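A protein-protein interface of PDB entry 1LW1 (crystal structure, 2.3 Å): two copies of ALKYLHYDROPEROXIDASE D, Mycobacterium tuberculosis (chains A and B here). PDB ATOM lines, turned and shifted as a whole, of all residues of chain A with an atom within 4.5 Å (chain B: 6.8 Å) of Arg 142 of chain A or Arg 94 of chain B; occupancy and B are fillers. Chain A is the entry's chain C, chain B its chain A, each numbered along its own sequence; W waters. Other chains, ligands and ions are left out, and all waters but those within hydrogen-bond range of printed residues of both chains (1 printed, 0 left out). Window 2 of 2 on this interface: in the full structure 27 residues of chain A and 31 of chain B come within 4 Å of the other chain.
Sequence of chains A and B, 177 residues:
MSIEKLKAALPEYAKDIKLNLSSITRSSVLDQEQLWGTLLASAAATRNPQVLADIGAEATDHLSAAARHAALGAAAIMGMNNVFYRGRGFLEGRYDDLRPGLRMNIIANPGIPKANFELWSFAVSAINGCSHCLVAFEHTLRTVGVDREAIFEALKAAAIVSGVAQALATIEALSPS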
ATOM      1  N   GLU A 138       6.697 -23.799  19.244  1.00  0.00           N
ATOM      2  CA  GLU A 138       7.115 -22.872  20.276  1.00  0.00           C
ATOM      3  C   GLU A 138       6.149 -22.984  21.467  1.00  0.00           C
ATOM      4  O   GLU A 138       6.527 -22.741  22.616  1.00  0.00           O
ATOM      5  CB  GLU A 138       7.126 -21.471  19.697  1.00  0.00           C
ATOM      6  CG  GLU A 138       7.578 -20.397  20.636  1.00  0.00           C
ATOM      7  CD  GLU A 138       6.507 -20.014  21.628  1.00  0.00           C
ATOM      8  OE1 GLU A 138       5.339 -19.817  21.210  1.00  0.00           O
ATOM      9  OE2 GLU A 138       6.844 -19.899  22.820  1.00  0.00           O
ATOM     10  N   HIS A 139       4.907 -23.371  21.192  1.00  0.00           N
ATOM     11  CA  HIS A 139       3.912 -23.532  22.258  1.00  0.00           C
ATOM     12  C   HIS A 139       4.172 -24.834  23.005  1.00  0.00           C
ATOM     13  O   HIS A 139       4.175 -24.859  24.234  1.00  0.00           O
ATOM     14  CB  HIS A 139       2.482 -23.547  21.694  1.00  0.00           C
ATOM     15  CG  HIS A 139       1.428 -23.785  22.731  1.00  0.00           C
ATOM     16  ND1 HIS A 139       1.148 -22.876  23.730  1.00  0.00           N
ATOM     17  CD2 HIS A 139       0.633 -24.858  22.963  1.00  0.00           C
ATOM     18  CE1 HIS A 139       0.231 -23.381  24.536  1.00  0.00           C
ATOM     19  NE2 HIS A 139      -0.098 -24.582  24.093  1.00  0.00           N
ATOM     20  N   THR A 140       4.387 -25.911  22.259  1.00  0.00           N
ATOM     21  CA  THR A 140       4.664 -27.209  22.863  1.00  0.00           C
ATOM     22  C   THR A 140       5.956 -27.169  23.683  1.00  0.00           C
ATOM     23  O   THR A 140       6.058 -27.787  24.740  1.00  0.00           O
ATOM     24  CB  THR A 140       4.829 -28.303  21.797  1.00  0.00           C
ATOM     25  OG1 THR A 140       3.682 -28.324  20.936  1.00  0.00           O
ATOM     26  CG2 THR A 140       5.012 -29.669  22.462  1.00  0.00           C
ATOM     27  N   LEU A 141       6.954 -26.454  23.182  1.00  0.00           N
ATOM     28  CA  LEU A 141       8.216 -26.362  23.886  1.00  0.00           C
ATOM     29  C   LEU A 141       8.043 -25.747  25.266  1.00  0.00           C
ATOM     30  O   LEU A 141       8.595 -26.248  26.243  1.00  0.00           O
ATOM     31  CB  LEU A 141       9.208 -25.549  23.067  1.00  0.00           C
ATOM     32  CG  LEU A 141       9.674 -26.302  21.820  1.00  0.00           C
ATOM     33  CD1 LEU A 141      10.594 -25.417  21.001  1.00  0.00           C
ATOM     34  CD2 LEU A 141      10.382 -27.592  22.235  1.00  0.00           C
ATOM     35  N   ARG A 142       7.275 -24.663  25.345  1.00  0.00           N
ATOM     36  CA  ARG A 142       7.035 -23.996  26.619  1.00  0.00           C
ATOM     37  C   ARG A 142       6.197 -24.887  27.530  1.00  0.00           C
ATOM     38  O   ARG A 142       6.422 -24.956  28.742  1.00  0.00           O
ATOM     39  CB  ARG A 142       6.327 -22.664  26.396  1.00  0.00           C
ATOM     40  CG  ARG A 142       7.222 -21.563  25.838  1.00  0.00           C
ATOM     41  CD  ARG A 142       6.441 -20.268  25.697  1.00  0.00           C
ATOM     42  NE  ARG A 142       5.249 -20.462  24.869  1.00  0.00           N
ATOM     43  CZ  ARG A 142       4.356 -19.517  24.585  1.00  0.00           C
ATOM     44  NH1 ARG A 142       4.503 -18.286  25.065  1.00  0.00           N
ATOM     45  NH2 ARG A 142       3.323 -19.807  23.805  1.00  0.00           N
ATOM     46  N   THR A 143       5.234 -25.575  26.934  1.00  0.00           N
ATOM     47  CA  THR A 143       4.370 -26.473  27.677  1.00  0.00           C
ATOM     48  C   THR A 143       5.145 -27.627  28.304  1.00  0.00           C
ATOM     49  O   THR A 143       4.795 -28.108  29.382  1.00  0.00           O
ATOM     50  CB  THR A 143       3.299 -27.058  26.770  1.00  0.00           C
ATOM     51  OG1 THR A 143       2.310 -26.060  26.500  1.00  0.00           O
ATOM     52  CG2 THR A 143       2.659 -28.277  27.420  1.00  0.00           C
ATOM     53  N   VAL A 144       6.199 -28.073  27.633  1.00  0.00           N
ATOM     54  CA  VAL A 144       6.991 -29.179  28.150  1.00  0.00           C
ATOM     55  C   VAL A 144       8.142 -28.695  29.021  1.00  0.00           C
ATOM     56  O   VAL A 144       8.946 -29.494  29.499  1.00  0.00           O
ATOM     57  CB  VAL A 144       7.527 -30.052  27.012  1.00  0.00           C
ATOM     58  CG1 VAL A 144       8.056 -31.360  27.564  1.00  0.00           C
ATOM     59  CG2 VAL A 144       6.419 -30.324  26.024  1.00  0.00           C
ATOM     60  N   GLY A 145       8.231 -27.379  29.208  1.00  0.00           N
ATOM     61  CA  GLY A 145       9.258 -26.823  30.080  1.00  0.00           C
ATOM     62  C   GLY A 145      10.584 -26.333  29.535  1.00  0.00           C
ATOM     63  O   GLY A 145      11.551 -26.201  30.293  1.00  0.00           O
ATOM     64  N   VAL A 146      10.641 -26.066  28.236  1.00  0.00           N
ATOM     65  CA  VAL A 146      11.856 -25.570  27.602  1.00  0.00           C
ATOM     66  C   VAL A 146      11.874 -24.054  27.813  1.00  0.00           C
ATOM     67  O   VAL A 146      10.882 -23.387  27.552  1.00  0.00           O
ATOM     68  CB  VAL A 146      11.858 -25.921  26.089  1.00  0.00           C
ATOM     69  CG1 VAL A 146      13.001 -25.240  25.390  1.00  0.00           C
ATOM     70  CG2 VAL A 146      11.991 -27.416  25.918  1.00  0.00           C
ATOM     71  N   ARG A 148      12.584 -19.998  27.467  1.00  0.00           N
ATOM     72  CA  ARG A 148      12.471 -19.039  26.368  1.00  0.00           C
ATOM     73  C   ARG A 148      13.828 -18.752  25.771  1.00  0.00           C
ATOM     74  O   ARG A 148      13.950 -18.473  24.582  1.00  0.00           O
ATOM     75  CB  ARG A 148      11.888 -17.703  26.859  1.00  0.00           C
ATOM     76  CG  ARG A 148      10.378 -17.639  27.018  1.00  0.00           C
ATOM     77  CD  ARG A 148       9.934 -16.306  27.647  1.00  0.00           C
ATOM     78  NE  ARG A 148      10.038 -15.143  26.760  1.00  0.00           N
ATOM     79  CZ  ARG A 148      10.873 -14.119  26.942  1.00  0.00           C
ATOM     80  NH1 ARG A 148      11.705 -14.095  27.979  1.00  0.00           N
ATOM     81  NH2 ARG A 148      10.856 -13.093  26.104  1.00  0.00           N
ATOM     82  N   ILE A 151      14.761 -21.505  23.437  1.00  0.00           N
ATOM     83  CA  ILE A 151      13.977 -21.438  22.212  1.00  0.00           C
ATOM     84  C   ILE A 151      14.564 -20.378  21.275  1.00  0.00           C
ATOM     85  O   ILE A 151      14.689 -20.591  20.072  1.00  0.00           O
ATOM     86  CB  ILE A 151      12.495 -21.142  22.560  1.00  0.00           C
ATOM     87  CG1 ILE A 151      11.898 -22.370  23.249  1.00  0.00           C
ATOM     88  CG2 ILE A 151      11.697 -20.788  21.306  1.00  0.00           C
ATOM     89  CD1 ILE A 151      10.520 -22.148  23.840  1.00  0.00           C
ATOM     90  N   ARG B  88      11.033 -13.770  14.912  1.00  0.00           N
ATOM     91  CA  ARG B  88      10.577 -12.964  16.032  1.00  0.00           C
ATOM     92  C   ARG B  88       9.172 -12.504  15.717  1.00  0.00           C
ATOM     93  O   ARG B  88       8.316 -12.506  16.586  1.00  0.00           O
ATOM     94  CB  ARG B  88      11.470 -11.745  16.237  1.00  0.00           C
ATOM     95  CG  ARG B  88      12.844 -12.092  16.747  1.00  0.00           C
ATOM     96  CD  ARG B  88      13.424 -10.945  17.549  1.00  0.00           C
ATOM     97  NE  ARG B  88      13.053  -9.654  16.981  1.00  0.00           N
ATOM     98  CZ  ARG B  88      13.570  -8.499  17.373  1.00  0.00           C
ATOM     99  NH1 ARG B  88      14.481  -8.475  18.329  1.00  0.00           N
ATOM    100  NH2 ARG B  88      13.180  -7.370  16.807  1.00  0.00           N
ATOM    101  N   PHE B  90       6.723 -13.913  13.965  1.00  0.00           N
ATOM    102  CA  PHE B  90       5.729 -14.960  14.214  1.00  0.00           C
ATOM    103  C   PHE B  90       5.467 -15.183  15.706  1.00  0.00           C
ATOM    104  O   PHE B  90       4.392 -15.642  16.091  1.00  0.00           O
ATOM    105  CB  PHE B  90       6.180 -16.293  13.606  1.00  0.00           C
ATOM    106  CG  PHE B  90       6.448 -16.240  12.122  1.00  0.00           C
ATOM    107  CD1 PHE B  90       5.852 -15.266  11.319  1.00  0.00           C
ATOM    108  CD2 PHE B  90       7.231 -17.226  11.513  1.00  0.00           C
ATOM    109  CE1 PHE B  90       6.025 -15.283   9.938  1.00  0.00           C
ATOM    110  CE2 PHE B  90       7.406 -17.249  10.138  1.00  0.00           C
ATOM    111  CZ  PHE B  90       6.800 -16.277   9.348  1.00  0.00           C
ATOM    112  N   LEU B  91       6.461 -14.885  16.535  1.00  0.00           N
ATOM    113  CA  LEU B  91       6.338 -15.052  17.980  1.00  0.00           C
ATOM    114  C   LEU B  91       5.819 -13.769  18.622  1.00  0.00           C
ATOM    115  O   LEU B  91       6.096 -13.477  19.784  1.00  0.00           O
ATOM    116  CB  LEU B  91       7.683 -15.429  18.595  1.00  0.00           C
ATOM    117  CG  LEU B  91       8.381 -16.655  18.024  1.00  0.00           C
ATOM    118  CD1 LEU B  91       9.729 -16.827  18.738  1.00  0.00           C
ATOM    119  CD2 LEU B  91       7.491 -17.887  18.175  1.00  0.00           C
ATOM    120  N   GLU B  92       5.089 -13.002  17.821  1.00  0.00           N
ATOM    121  CA  GLU B  92       4.449 -11.765  18.237  1.00  0.00           C
ATOM    122  C   GLU B  92       5.237 -10.903  19.208  1.00  0.00           C
ATOM    123  O   GLU B  92       4.684 -10.363  20.168  1.00  0.00           O
ATOM    124  CB  GLU B  92       3.080 -12.106  18.823  1.00  0.00           C
ATOM    125  CG  GLU B  92       2.204 -12.859  17.845  1.00  0.00           C
ATOM    126  CD  GLU B  92       1.067 -13.581  18.518  1.00  0.00           C
ATOM    127  OE1 GLU B  92       0.163 -12.911  19.058  1.00  0.00           O
ATOM    128  OE2 GLU B  92       1.085 -14.829  18.513  1.00  0.00           O
ATOM    129  N   GLY B  93       6.530 -10.768  18.954  1.00  0.00           N
ATOM    130  CA  GLY B  93       7.358  -9.942  19.808  1.00  0.00           C
ATOM    131  C   GLY B  93       7.660 -10.499  21.185  1.00  0.00           C
ATOM    132  O   GLY B  93       8.385  -9.863  21.939  1.00  0.00           O
ATOM    133  N   ARG B  94       7.117 -11.668  21.515  1.00  0.00           N
ATOM    134  CA  ARG B  94       7.352 -12.289  22.823  1.00  0.00           C
ATOM    135  C   ARG B  94       8.829 -12.398  23.191  1.00  0.00           C
ATOM    136  O   ARG B  94       9.156 -12.650  24.347  1.00  0.00           O
ATOM    137  CB  ARG B  94       6.761 -13.700  22.880  1.00  0.00           C
ATOM    138  CG  ARG B  94       5.255 -13.784  22.946  1.00  0.00           C
ATOM    139  CD  ARG B  94       4.827 -15.125  23.547  1.00  0.00           C
ATOM    140  NE  ARG B  94       4.932 -16.228  22.600  1.00  0.00           N
ATOM    141  CZ  ARG B  94       4.166 -16.360  21.517  1.00  0.00           C
ATOM    142  NH1 ARG B  94       3.234 -15.462  21.238  1.00  0.00           N
ATOM    143  NH2 ARG B  94       4.339 -17.395  20.703  1.00  0.00           N
ATOM    144  N   TYR B  95       9.719 -12.224  22.214  1.00  0.00           N
ATOM    145  CA  TYR B  95      11.159 -12.330  22.468  1.00  0.00           C
ATOM    146  C   TYR B  95      11.939 -11.080  22.072  1.00  0.00           C
ATOM    147  O   TYR B  95      13.174 -11.093  22.033  1.00  0.00           O
ATOM    148  CB  TYR B  95      11.737 -13.541  21.731  1.00  0.00           C
ATOM    149  CG  TYR B  95      11.175 -14.882  22.164  1.00  0.00           C
ATOM    150  CD1 TYR B  95       9.836 -15.211  21.945  1.00  0.00           C
ATOM    151  CD2 TYR B  95      11.991 -15.833  22.773  1.00  0.00           C
ATOM    152  CE1 TYR B  95       9.330 -16.456  22.322  1.00  0.00           C
ATOM    153  CE2 TYR B  95      11.498 -17.076  23.153  1.00  0.00           C
ATOM    154  CZ  TYR B  95      10.166 -17.382  22.928  1.00  0.00           C
ATOM    155  OH  TYR B  95       9.676 -18.609  23.334  1.00  0.00           O
ATOM    156  N   ASP B  96      11.219 -10.002  21.784  1.00  0.00           N
ATOM    157  CA  ASP B  96      11.836  -8.738  21.400  1.00  0.00           C
ATOM    158  C   ASP B  96      12.751  -8.190  22.490  1.00  0.00           C
ATOM    159  O   ASP B  96      13.446  -7.197  22.287  1.00  0.00           O
ATOM    160  CB  ASP B  96      10.753  -7.707  21.089  1.00  0.00           C
ATOM    161  CG  ASP B  96      10.220  -7.830  19.680  1.00  0.00           C
ATOM    162  OD1 ASP B  96      10.061  -8.969  19.198  1.00  0.00           O
ATOM    163  OD2 ASP B  96       9.949  -6.781  19.056  1.00  0.00           O
ATOM    164  N   ASP B  97      12.758  -8.840  23.644  1.00  0.00           N
ATOM    165  CA  ASP B  97      13.585  -8.376  24.745  1.00  0.00           C
ATOM    166  C   ASP B  97      14.627  -9.386  25.208  1.00  0.00           C
ATOM    167  O   ASP B  97      14.769  -9.613  26.408  1.00  0.00           O
ATOM    168  CB  ASP B  97      12.692  -7.996  25.916  1.00  0.00           C
ATOM    169  CG  ASP B  97      11.755  -9.112  26.302  1.00  0.00           C
ATOM    170  OD1 ASP B  97      10.543  -8.839  26.451  1.00  0.00           O
ATOM    171  OD2 ASP B  97      12.229 -10.262  26.452  1.00  0.00           O
ATOM    172  N   LEU B  98      15.353  -9.993  24.275  1.00  0.00           N
ATOM    173  CA  LEU B  98      16.378 -10.958  24.648  1.00  0.00           C
ATOM    174  C   LEU B  98      17.750 -10.665  24.080  1.00  0.00           C
ATOM    175  O   LEU B  98      18.624 -11.530  24.132  1.00  0.00           O
ATOM    176  CB  LEU B  98      15.981 -12.373  24.231  1.00  0.00           C
ATOM    177  CG  LEU B  98      14.932 -13.072  25.091  1.00  0.00           C
ATOM    178  CD1 LEU B  98      13.577 -12.423  24.854  1.00  0.00           C
ATOM    179  CD2 LEU B  98      14.891 -14.544  24.745  1.00  0.00           C
HETATM  180  O   HOH W   1       7.625 -12.362  27.040  1.00  0.00           O
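The guanidinium group (NH2) of Arg 94 of chain B lies within salt-bridge range of the side-chain carboxylate (OE1) of Glu 138 of chain A, 2.7 Å away.
NH2 of Arg 148 of chain A sits at hydrogen-bond distance from O of Arg 94 of chain B.
The side-chain hydroxyl (OH) of Tyr 95 of chain B lies within hydrogen-bond range of the side-chain carboxylate (OE2) of Glu 138 of chain A (3.2 Å).
The side-chain carboxylate (OD2) of Asp 97 of chain B is in salt-bridge range of the guanidinium group (NH2) of Arg 148 of chain A (3.2 Å).
NE of Arg 94 of chain B sits close to NH1 of Arg 142 of chain A (3.2 Å).
OE2 of Glu 92 of chain B is in salt-bridge range of NH1 of Arg 94 of chain B (3.5 Å).
The side-chain carboxylate (OE2) of Glu 138 of chain A is in salt-bridge range of the guanidinium group (NE) of Arg 142 of chain A (2.7 Å).
Among the printed residues, pairs that only touch across the chains: Arg 148 of chain A with Leu 98 of chain B, Arg 148 of chain A with Tyr 95 of chain B, Glu 138 of chain A with Leu 91 of chain B and Ile 151 of chain A with Tyr 95 of chain B.
Of the printed residues of chain B, Glu 138 of chain A touches Leu 91 (3.5 Å), Arg 94 (2.7 Å) and Tyr 95 (3.2 Å).
Thr 140 of chain A touches none of the printed residues of chain B.
Of chain B, only Arg 94 comes within 4 Å of Arg 142 of chain A.
Printed residues of chain B within 4 Å of Arg 148 of chain A: Arg 94, Tyr 95, Asp 97 and Leu 98.
Glu 92 of chain B touches none of the printed residues of chain A.
Of the printed residues of chain A, Tyr 95 of chain B touches Glu 138 (3.2 Å), Arg 148 (3.2 Å) and Ile 151 (3.6 Å).
Of the printed residues of chain A, Asp 97 of chain B touches Arg 148.
Printed residues of chain A within 4 Å of Leu 98 of chain B: Arg 148 (3.1 Å).
The nearest printed residue of chain A that does not touch Arg 94 of chain B is His 139 of chain A (6.0 Å).
The nearest printed residue of chain B that does not touch Glu 138 of chain A is Phe 90 of chain B (6.7 Å).
Of the 11 printed residues of chain A, 4 touch a printed residue of chain B.
Hydrophobic or aromatic side chains of chain A within 4 Å of the printed part of chain B: Ile 151.
Along chain A the printed residues that touch a printed residue of chain B span positions 138 to 151.
Among the printed residues, 9 pairs touch across the chains.
Among the printed residues, Asp or Glu carboxylates within 4 Å of a Lys or Arg side-chain nitrogen of the other chain: Glu 138 of chain A with Arg 94 of chain B and Arg 148 of chain A with Asp 97 of chain B.
No position is printed for both chains.
Of the 9 pairs that touch across the chains among the printed residues, none has its exchanged pair printed and touching as well.
Water W1 lies within hydrogen-bond range of O of Arg 94 of chain B (3.1 Å) and NH2 of Arg 148 of chain A (3.4 Å).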
